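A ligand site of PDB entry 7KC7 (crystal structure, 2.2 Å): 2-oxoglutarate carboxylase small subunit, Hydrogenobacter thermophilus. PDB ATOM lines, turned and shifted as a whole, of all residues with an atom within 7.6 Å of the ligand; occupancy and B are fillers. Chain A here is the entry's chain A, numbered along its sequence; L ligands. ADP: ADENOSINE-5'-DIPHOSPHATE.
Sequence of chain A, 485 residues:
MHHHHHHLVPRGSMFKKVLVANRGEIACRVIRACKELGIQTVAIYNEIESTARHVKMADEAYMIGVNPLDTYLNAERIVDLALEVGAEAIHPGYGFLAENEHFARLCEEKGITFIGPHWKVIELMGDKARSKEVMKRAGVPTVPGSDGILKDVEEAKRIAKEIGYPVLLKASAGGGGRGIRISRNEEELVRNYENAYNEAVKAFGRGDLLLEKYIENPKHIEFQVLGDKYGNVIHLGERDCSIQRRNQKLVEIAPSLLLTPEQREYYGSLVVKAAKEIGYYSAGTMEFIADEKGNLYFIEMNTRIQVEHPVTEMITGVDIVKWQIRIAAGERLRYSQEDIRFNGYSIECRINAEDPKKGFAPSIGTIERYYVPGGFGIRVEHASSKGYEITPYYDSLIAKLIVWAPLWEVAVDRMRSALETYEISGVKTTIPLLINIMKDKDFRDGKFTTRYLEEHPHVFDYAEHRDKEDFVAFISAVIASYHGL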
ATOM      1  N   LYS A 128      -9.205  23.581  15.160  1.00  0.00           N
ATOM      2  CA  LYS A 128      -9.573  23.662  13.743  1.00  0.00           C
ATOM      3  C   LYS A 128      -8.445  23.123  12.831  1.00  0.00           C
ATOM      4  O   LYS A 128      -8.735  22.522  11.788  1.00  0.00           O
ATOM      5  CB  LYS A 128      -9.913  25.114  13.376  1.00  0.00           C
ATOM      6  CG  LYS A 128     -11.323  25.369  13.950  1.00  0.00           C
ATOM      7  CD  LYS A 128     -11.671  26.843  14.025  1.00  0.00           C
ATOM      8  CE  LYS A 128     -13.158  27.121  14.198  1.00  0.00           C
ATOM      9  NZ  LYS A 128     -13.242  28.472  13.671  1.00  0.00           N
ATOM     10  N   LYS A 132      -8.876  19.803  10.524  1.00  0.00           N
ATOM     11  CA  LYS A 132      -8.688  19.914   9.082  1.00  0.00           C
ATOM     12  C   LYS A 132      -7.680  18.858   8.576  1.00  0.00           C
ATOM     13  O   LYS A 132      -7.894  18.223   7.536  1.00  0.00           O
ATOM     14  CB  LYS A 132      -8.231  21.338   8.805  1.00  0.00           C
ATOM     15  CG  LYS A 132      -8.247  21.720   7.377  1.00  0.00           C
ATOM     16  CD  LYS A 132      -7.968  23.183   7.207  1.00  0.00           C
ATOM     17  CE  LYS A 132      -7.238  23.384   5.893  1.00  0.00           C
ATOM     18  NZ  LYS A 132      -7.454  24.751   5.423  1.00  0.00           N
ATOM     19  N   VAL A 143     -10.269  23.600   2.392  1.00  0.00           N
ATOM     20  CA  VAL A 143      -9.908  24.845   1.703  1.00  0.00           C
ATOM     21  C   VAL A 143      -8.390  24.952   1.587  1.00  0.00           C
ATOM     22  O   VAL A 143      -7.705  24.815   2.615  1.00  0.00           O
ATOM     23  CB  VAL A 143     -10.491  26.053   2.446  1.00  0.00           C
ATOM     24  CG1 VAL A 143     -10.182  27.328   1.668  1.00  0.00           C
ATOM     25  CG2 VAL A 143     -12.018  25.900   2.682  1.00  0.00           C
ATOM     26  N   PRO A 144      -7.830  25.240   0.405  1.00  0.00           N
ATOM     27  CA  PRO A 144      -6.365  25.372   0.311  1.00  0.00           C
ATOM     28  C   PRO A 144      -5.873  26.406   1.303  1.00  0.00           C
ATOM     29  O   PRO A 144      -6.502  27.447   1.505  1.00  0.00           O
ATOM     30  CB  PRO A 144      -6.140  25.859  -1.128  1.00  0.00           C
ATOM     31  CG  PRO A 144      -7.341  25.408  -1.912  1.00  0.00           C
ATOM     32  CD  PRO A 144      -8.471  25.127  -0.923  1.00  0.00           C
ATOM     33  N   VAL A 167      -7.426  36.215   1.200  1.00  0.00           N
ATOM     34  CA  VAL A 167      -7.165  35.114   2.119  1.00  0.00           C
ATOM     35  C   VAL A 167      -7.774  35.397   3.483  1.00  0.00           C
ATOM     36  O   VAL A 167      -8.120  36.543   3.820  1.00  0.00           O
ATOM     37  CB  VAL A 167      -5.651  34.800   2.275  1.00  0.00           C
ATOM     38  CG1 VAL A 167      -5.067  34.461   0.920  1.00  0.00           C
ATOM     39  CG2 VAL A 167      -4.911  35.923   2.906  1.00  0.00           C
ATOM     40  N   LEU A 168      -7.863  34.336   4.296  1.00  0.00           N
ATOM     41  CA  LEU A 168      -8.560  34.347   5.575  1.00  0.00           C
ATOM     42  C   LEU A 168      -7.650  33.916   6.715  1.00  0.00           C
ATOM     43  O   LEU A 168      -6.948  32.911   6.606  1.00  0.00           O
ATOM     44  CB  LEU A 168      -9.759  33.395   5.555  1.00  0.00           C
ATOM     45  CG  LEU A 168     -10.860  33.446   6.625  1.00  0.00           C
ATOM     46  CD1 LEU A 168     -11.346  34.926   6.787  1.00  0.00           C
ATOM     47  CD2 LEU A 168     -11.992  32.438   6.291  1.00  0.00           C
ATOM     48  N   LYS A 170      -7.865  32.500  10.678  1.00  0.00           N
ATOM     49  CA  LYS A 170      -8.815  31.956  11.628  1.00  0.00           C
ATOM     50  C   LYS A 170      -8.120  31.500  12.895  1.00  0.00           C
ATOM     51  O   LYS A 170      -7.068  30.857  12.834  1.00  0.00           O
ATOM     52  CB  LYS A 170      -9.518  30.678  11.137  1.00  0.00           C
ATOM     53  CG  LYS A 170     -10.569  30.739  10.096  1.00  0.00           C
ATOM     54  CD  LYS A 170     -11.129  29.303  10.002  1.00  0.00           C
ATOM     55  CE  LYS A 170     -12.106  29.125   8.891  1.00  0.00           C
ATOM     56  NZ  LYS A 170     -12.328  27.685   8.686  1.00  0.00           N
ATOM     57  N   ILE A 180     -11.147  36.149  13.581  1.00  0.00           N
ATOM     58  CA  ILE A 180     -11.149  36.026  12.118  1.00  0.00           C
ATOM     59  C   ILE A 180     -11.027  37.375  11.412  1.00  0.00           C
ATOM     60  O   ILE A 180     -11.683  38.353  11.775  1.00  0.00           O
ATOM     61  CB  ILE A 180     -12.425  35.321  11.637  1.00  0.00           C
ATOM     62  CG1 ILE A 180     -12.508  33.874  12.163  1.00  0.00           C
ATOM     63  CG2 ILE A 180     -12.549  35.425  10.139  1.00  0.00           C
ATOM     64  CD1 ILE A 180     -13.999  33.279  11.824  1.00  0.00           C
ATOM     65  N   ILE A 182     -10.300  39.059   7.130  1.00  0.00           N
ATOM     66  CA  ILE A 182     -10.126  38.871   5.690  1.00  0.00           C
ATOM     67  C   ILE A 182      -9.014  39.821   5.246  1.00  0.00           C
ATOM     68  O   ILE A 182      -9.009  40.995   5.594  1.00  0.00           O
ATOM     69  CB  ILE A 182     -11.424  39.141   4.899  1.00  0.00           C
ATOM     70  CG1 ILE A 182     -12.594  38.279   5.404  1.00  0.00           C
ATOM     71  CG2 ILE A 182     -11.210  38.869   3.412  1.00  0.00           C
ATOM     72  CD1 ILE A 182     -13.853  38.577   4.659  1.00  0.00           C
ATOM     73  N   GLU A 212      -6.231  30.272   5.218  1.00  0.00           N
ATOM     74  CA  GLU A 212      -6.806  29.530   4.129  1.00  0.00           C
ATOM     75  C   GLU A 212      -7.318  30.594   3.179  1.00  0.00           C
ATOM     76  O   GLU A 212      -7.230  31.786   3.494  1.00  0.00           O
ATOM     77  CB  GLU A 212      -7.890  28.549   4.596  1.00  0.00           C
ATOM     78  CG  GLU A 212      -9.142  29.074   5.293  1.00  0.00           C
ATOM     79  CD  GLU A 212     -10.043  27.900   5.789  1.00  0.00           C
ATOM     80  OE1 GLU A 212      -9.549  26.754   6.009  1.00  0.00           O
ATOM     81  OE2 GLU A 212     -11.252  28.125   5.947  1.00  0.00           O
ATOM     82  N   LYS A 213      -8.099  30.192   2.203  1.00  0.00           N
ATOM     83  CA  LYS A 213      -8.207  31.018   1.033  1.00  0.00           C
ATOM     84  C   LYS A 213      -9.631  31.436   1.158  1.00  0.00           C
ATOM     85  O   LYS A 213     -10.441  30.654   1.638  1.00  0.00           O
ATOM     86  CB  LYS A 213      -7.924  30.243  -0.233  1.00  0.00           C
ATOM     87  CG  LYS A 213      -7.945  31.158  -1.419  1.00  0.00           C
ATOM     88  CD  LYS A 213      -8.126  30.498  -2.774  1.00  0.00           C
ATOM     89  CE  LYS A 213      -8.084  31.599  -3.870  1.00  0.00           C
ATOM     90  NZ  LYS A 213      -6.747  31.885  -4.538  1.00  0.00           N
ATOM     91  N   TYR A 214      -9.958  32.635   0.751  1.00  0.00           N
ATOM     92  CA  TYR A 214     -11.230  33.149   1.165  1.00  0.00           C
ATOM     93  C   TYR A 214     -12.243  32.993   0.052  1.00  0.00           C
ATOM     94  O   TYR A 214     -12.046  33.482  -1.065  1.00  0.00           O
ATOM     95  CB  TYR A 214     -11.118  34.615   1.515  1.00  0.00           C
ATOM     96  CG  TYR A 214     -12.444  35.235   1.827  1.00  0.00           C
ATOM     97  CD1 TYR A 214     -13.230  34.783   2.869  1.00  0.00           C
ATOM     98  CD2 TYR A 214     -12.922  36.290   1.054  1.00  0.00           C
ATOM     99  CE1 TYR A 214     -14.447  35.391   3.161  1.00  0.00           C
ATOM    100  CE2 TYR A 214     -14.115  36.881   1.329  1.00  0.00           C
ATOM    101  CZ  TYR A 214     -14.892  36.426   2.370  1.00  0.00           C
ATOM    102  OH  TYR A 214     -16.092  37.030   2.647  1.00  0.00           O
ATOM    103  N   ILE A 215     -13.335  32.325   0.401  1.00  0.00           N
ATOM    104  CA  ILE A 215     -14.417  32.000  -0.503  1.00  0.00           C
ATOM    105  C   ILE A 215     -15.527  32.997  -0.250  1.00  0.00           C
ATOM    106  O   ILE A 215     -16.173  33.014   0.806  1.00  0.00           O
ATOM    107  CB  ILE A 215     -14.866  30.557  -0.310  1.00  0.00           C
ATOM    108  CG1 ILE A 215     -13.702  29.659  -0.746  1.00  0.00           C
ATOM    109  CG2 ILE A 215     -16.163  30.262  -1.111  1.00  0.00           C
ATOM    110  CD1 ILE A 215     -14.027  28.266  -1.254  1.00  0.00           C
ATOM    111  N   GLU A 216     -15.725  33.831  -1.250  1.00  0.00           N
ATOM    112  CA  GLU A 216     -16.746  34.851  -1.164  1.00  0.00           C
ATOM    113  C   GLU A 216     -18.075  34.208  -1.526  1.00  0.00           C
ATOM    114  O   GLU A 216     -18.138  33.218  -2.263  1.00  0.00           O
ATOM    115  CB  GLU A 216     -16.400  35.948  -2.172  1.00  0.00           C
ATOM    116  CG  GLU A 216     -15.115  36.649  -1.846  1.00  0.00           C
ATOM    117  CD  GLU A 216     -14.639  37.565  -2.947  1.00  0.00           C
ATOM    118  OE1 GLU A 216     -14.996  38.765  -2.991  1.00  0.00           O
ATOM    119  OE2 GLU A 216     -13.841  37.028  -3.759  1.00  0.00           O
ATOM    120  N   ASN A 217     -19.134  34.733  -0.975  1.00  0.00           N
ATOM    121  CA  ASN A 217     -20.451  34.208  -1.246  1.00  0.00           C
ATOM    122  C   ASN A 217     -20.671  32.690  -1.173  1.00  0.00           C
ATOM    123  O   ASN A 217     -21.329  32.119  -2.036  1.00  0.00           O
ATOM    124  CB  ASN A 217     -20.804  34.722  -2.640  1.00  0.00           C
ATOM    125  CG  ASN A 217     -22.260  34.792  -2.883  1.00  0.00           C
ATOM    126  OD1 ASN A 217     -23.049  35.220  -2.023  1.00  0.00           O
ATOM    127  ND2 ASN A 217     -22.670  34.362  -4.081  1.00  0.00           N
ATOM    128  N   PRO A 218     -20.208  32.034  -0.120  1.00  0.00           N
ATOM    129  CA  PRO A 218     -20.368  30.583  -0.062  1.00  0.00           C
ATOM    130  C   PRO A 218     -21.749  30.182   0.459  1.00  0.00           C
ATOM    131  O   PRO A 218     -22.412  30.901   1.205  1.00  0.00           O
ATOM    132  CB  PRO A 218     -19.299  30.152   0.928  1.00  0.00           C
ATOM    133  CG  PRO A 218     -19.253  31.271   1.906  1.00  0.00           C
ATOM    134  CD  PRO A 218     -19.453  32.539   1.045  1.00  0.00           C
ATOM    135  N   HIS A 220     -23.479  27.241   2.988  1.00  0.00           N
ATOM    136  CA  HIS A 220     -23.113  26.482   4.180  1.00  0.00           C
ATOM    137  C   HIS A 220     -23.868  25.158   4.062  1.00  0.00           C
ATOM    138  O   HIS A 220     -25.114  25.149   4.120  1.00  0.00           O
ATOM    139  CB  HIS A 220     -23.507  27.215   5.482  1.00  0.00           C
ATOM    140  CG  HIS A 220     -23.024  26.522   6.732  1.00  0.00           C
ATOM    141  ND1 HIS A 220     -23.552  25.340   7.191  1.00  0.00           N
ATOM    142  CD2 HIS A 220     -22.053  26.870   7.627  1.00  0.00           C
ATOM    143  CE1 HIS A 220     -22.907  24.951   8.281  1.00  0.00           C
ATOM    144  NE2 HIS A 220     -22.000  25.873   8.574  1.00  0.00           N
ATOM    145  N   ILE A 289     -18.246  24.663   3.477  1.00  0.00           N
ATOM    146  CA  ILE A 289     -18.655  25.765   2.615  1.00  0.00           C
ATOM    147  C   ILE A 289     -18.593  25.254   1.191  1.00  0.00           C
ATOM    148  O   ILE A 289     -17.779  24.383   0.872  1.00  0.00           O
ATOM    149  CB  ILE A 289     -17.795  27.020   2.819  1.00  0.00           C
ATOM    150  CG1 ILE A 289     -16.311  26.682   2.815  1.00  0.00           C
ATOM    151  CG2 ILE A 289     -18.158  27.744   4.125  1.00  0.00           C
ATOM    152  CD1 ILE A 289     -15.412  27.905   2.999  1.00  0.00           C
ATOM    153  N   TYR A 297     -15.897  22.261   0.608  1.00  0.00           N
ATOM    154  CA  TYR A 297     -14.688  22.301   1.398  1.00  0.00           C
ATOM    155  C   TYR A 297     -15.054  22.254   2.867  1.00  0.00           C
ATOM    156  O   TYR A 297     -15.847  23.090   3.332  1.00  0.00           O
ATOM    157  CB  TYR A 297     -13.908  23.587   1.078  1.00  0.00           C
ATOM    158  CG  TYR A 297     -13.691  23.827  -0.406  1.00  0.00           C
ATOM    159  CD1 TYR A 297     -14.654  24.485  -1.155  1.00  0.00           C
ATOM    160  CD2 TYR A 297     -12.511  23.416  -1.048  1.00  0.00           C
ATOM    161  CE1 TYR A 297     -14.481  24.701  -2.511  1.00  0.00           C
ATOM    162  CE2 TYR A 297     -12.320  23.658  -2.404  1.00  0.00           C
ATOM    163  CZ  TYR A 297     -13.305  24.289  -3.122  1.00  0.00           C
ATOM    164  OH  TYR A 297     -13.116  24.510  -4.460  1.00  0.00           O
ATOM    165  N   PHE A 298     -14.483  21.268   3.580  1.00  0.00           N
ATOM    166  CA  PHE A 298     -14.626  21.121   5.030  1.00  0.00           C
ATOM    167  C   PHE A 298     -14.065  22.349   5.724  1.00  0.00           C
ATOM    168  O   PHE A 298     -13.157  22.988   5.201  1.00  0.00           O
ATOM    169  CB  PHE A 298     -13.874  19.862   5.518  1.00  0.00           C
ATOM    170  CG  PHE A 298     -13.857  19.716   7.021  1.00  0.00           C
ATOM    171  CD1 PHE A 298     -14.888  19.045   7.665  1.00  0.00           C
ATOM    172  CD2 PHE A 298     -12.797  20.211   7.783  1.00  0.00           C
ATOM    173  CE1 PHE A 298     -14.898  18.905   9.031  1.00  0.00           C
ATOM    174  CE2 PHE A 298     -12.788  20.054   9.164  1.00  0.00           C
ATOM    175  CZ  PHE A 298     -13.865  19.419   9.790  1.00  0.00           C
ATOM    176  N   ILE A 299     -14.669  22.759   6.835  1.00  0.00           N
ATOM    177  CA  ILE A 299     -14.119  23.837   7.638  1.00  0.00           C
ATOM    178  C   ILE A 299     -14.133  23.524   9.129  1.00  0.00           C
ATOM    179  O   ILE A 299     -13.331  24.077   9.892  1.00  0.00           O
ATOM    180  CB  ILE A 299     -14.823  25.176   7.364  1.00  0.00           C
ATOM    181  CG1 ILE A 299     -16.333  25.035   7.465  1.00  0.00           C
ATOM    182  CG2 ILE A 299     -14.469  25.724   6.001  1.00  0.00           C
ATOM    183  CD1 ILE A 299     -17.062  26.378   7.472  1.00  0.00           C
ATOM    184  N   GLU A 300     -15.132  22.769   9.584  1.00  0.00           N
ATOM    185  CA  GLU A 300     -15.096  22.423  11.002  1.00  0.00           C
ATOM    186  C   GLU A 300     -16.125  21.370  11.329  1.00  0.00           C
ATOM    187  O   GLU A 300     -17.007  21.031  10.541  1.00  0.00           O
ATOM    188  CB  GLU A 300     -15.248  23.682  11.857  1.00  0.00           C
ATOM    189  CG  GLU A 300     -16.637  24.243  12.051  1.00  0.00           C
ATOM    190  CD  GLU A 300     -16.614  25.466  12.974  1.00  0.00           C
ATOM    191  OE1 GLU A 300     -17.465  25.585  13.873  1.00  0.00           O
ATOM    192  OE2 GLU A 300     -15.748  26.342  12.779  1.00  0.00           O
ATOM    193  N   THR A 450     -24.728  32.310   2.227  1.00  0.00           N
ATOM    194  CA  THR A 450     -24.527  32.936   3.523  1.00  0.00           C
ATOM    195  C   THR A 450     -24.719  34.430   3.501  1.00  0.00           C
ATOM    196  O   THR A 450     -24.813  35.042   4.574  1.00  0.00           O
ATOM    197  CB  THR A 450     -23.132  32.608   4.047  1.00  0.00           C
ATOM    198  OG1 THR A 450     -22.132  33.032   3.096  1.00  0.00           O
ATOM    199  CG2 THR A 450     -23.017  31.146   4.320  1.00  0.00           C
HETATM  200  N9  ADP L   1     -15.722  30.613   6.946  1.00  0.00           N
HETATM  201  C8  ADP L   1     -14.749  29.760   7.357  1.00  0.00           C
HETATM  202  N7  ADP L   1     -13.802  29.583   6.393  1.00  0.00           N
HETATM  203  C5  ADP L   1     -14.212  30.338   5.351  1.00  0.00           C
HETATM  204  C6  ADP L   1     -13.681  30.600   4.018  1.00  0.00           C
HETATM  205  N6  ADP L   1     -12.542  29.987   3.668  1.00  0.00           N
HETATM  206  N1  ADP L   1     -14.362  31.426   3.205  1.00  0.00           N
HETATM  207  C2  ADP L   1     -15.504  32.018   3.574  1.00  0.00           C
HETATM  208  N3  ADP L   1     -16.072  31.825   4.788  1.00  0.00           N
HETATM  209  C4  ADP L   1     -15.470  31.019   5.699  1.00  0.00           C
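Leu 168 touches the ligand (CD2 to C5, 3.2 Å). Tyr 214 touches the ligand. Ile 289 touches the ligand. Ile 299 touches the ligand (CG2 to N7, 3.9 Å). Of the 23 residues printed, 8 come within 4 Å of the ligand.
OE2 of Glu 212 lies within salt-bridge range of NZ of Lys 170. The backbone carbonyl oxygen of Glu 212 lies within hydrogen-bond range of the backbone NH of Leu 168 (2.7 Å). The side-chain carboxylate (OE1) of Glu 212 is in salt-bridge range of the side-chain amino group (NZ) of Lys 132 (3.0 Å). The backbone carbonyl oxygen (O) of Pro 144 sits at hydrogen-bond distance from the backbone NH (N) of Lys 213 (3.3 Å). The backbone NH of Tyr 297 is in hydrogen-bond range of the backbone carbonyl oxygen of Ile 289 (2.8 Å).
A nitrogen (N6) of the ligand is in hydrogen-bond range of the side-chain carboxylate of Glu 212 (3.2 Å). A nitrogen (N6) of the ligand is in hydrogen-bond range of the backbone carbonyl oxygen of Lys 213 (3.0 Å). N of Ile 215 lies within hydrogen-bond range of N1 of the ligand, at 3.1 Å. A nitrogen (N7) of the ligand sits close to the side-chain amino group of Lys 170 (3.3 Å).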
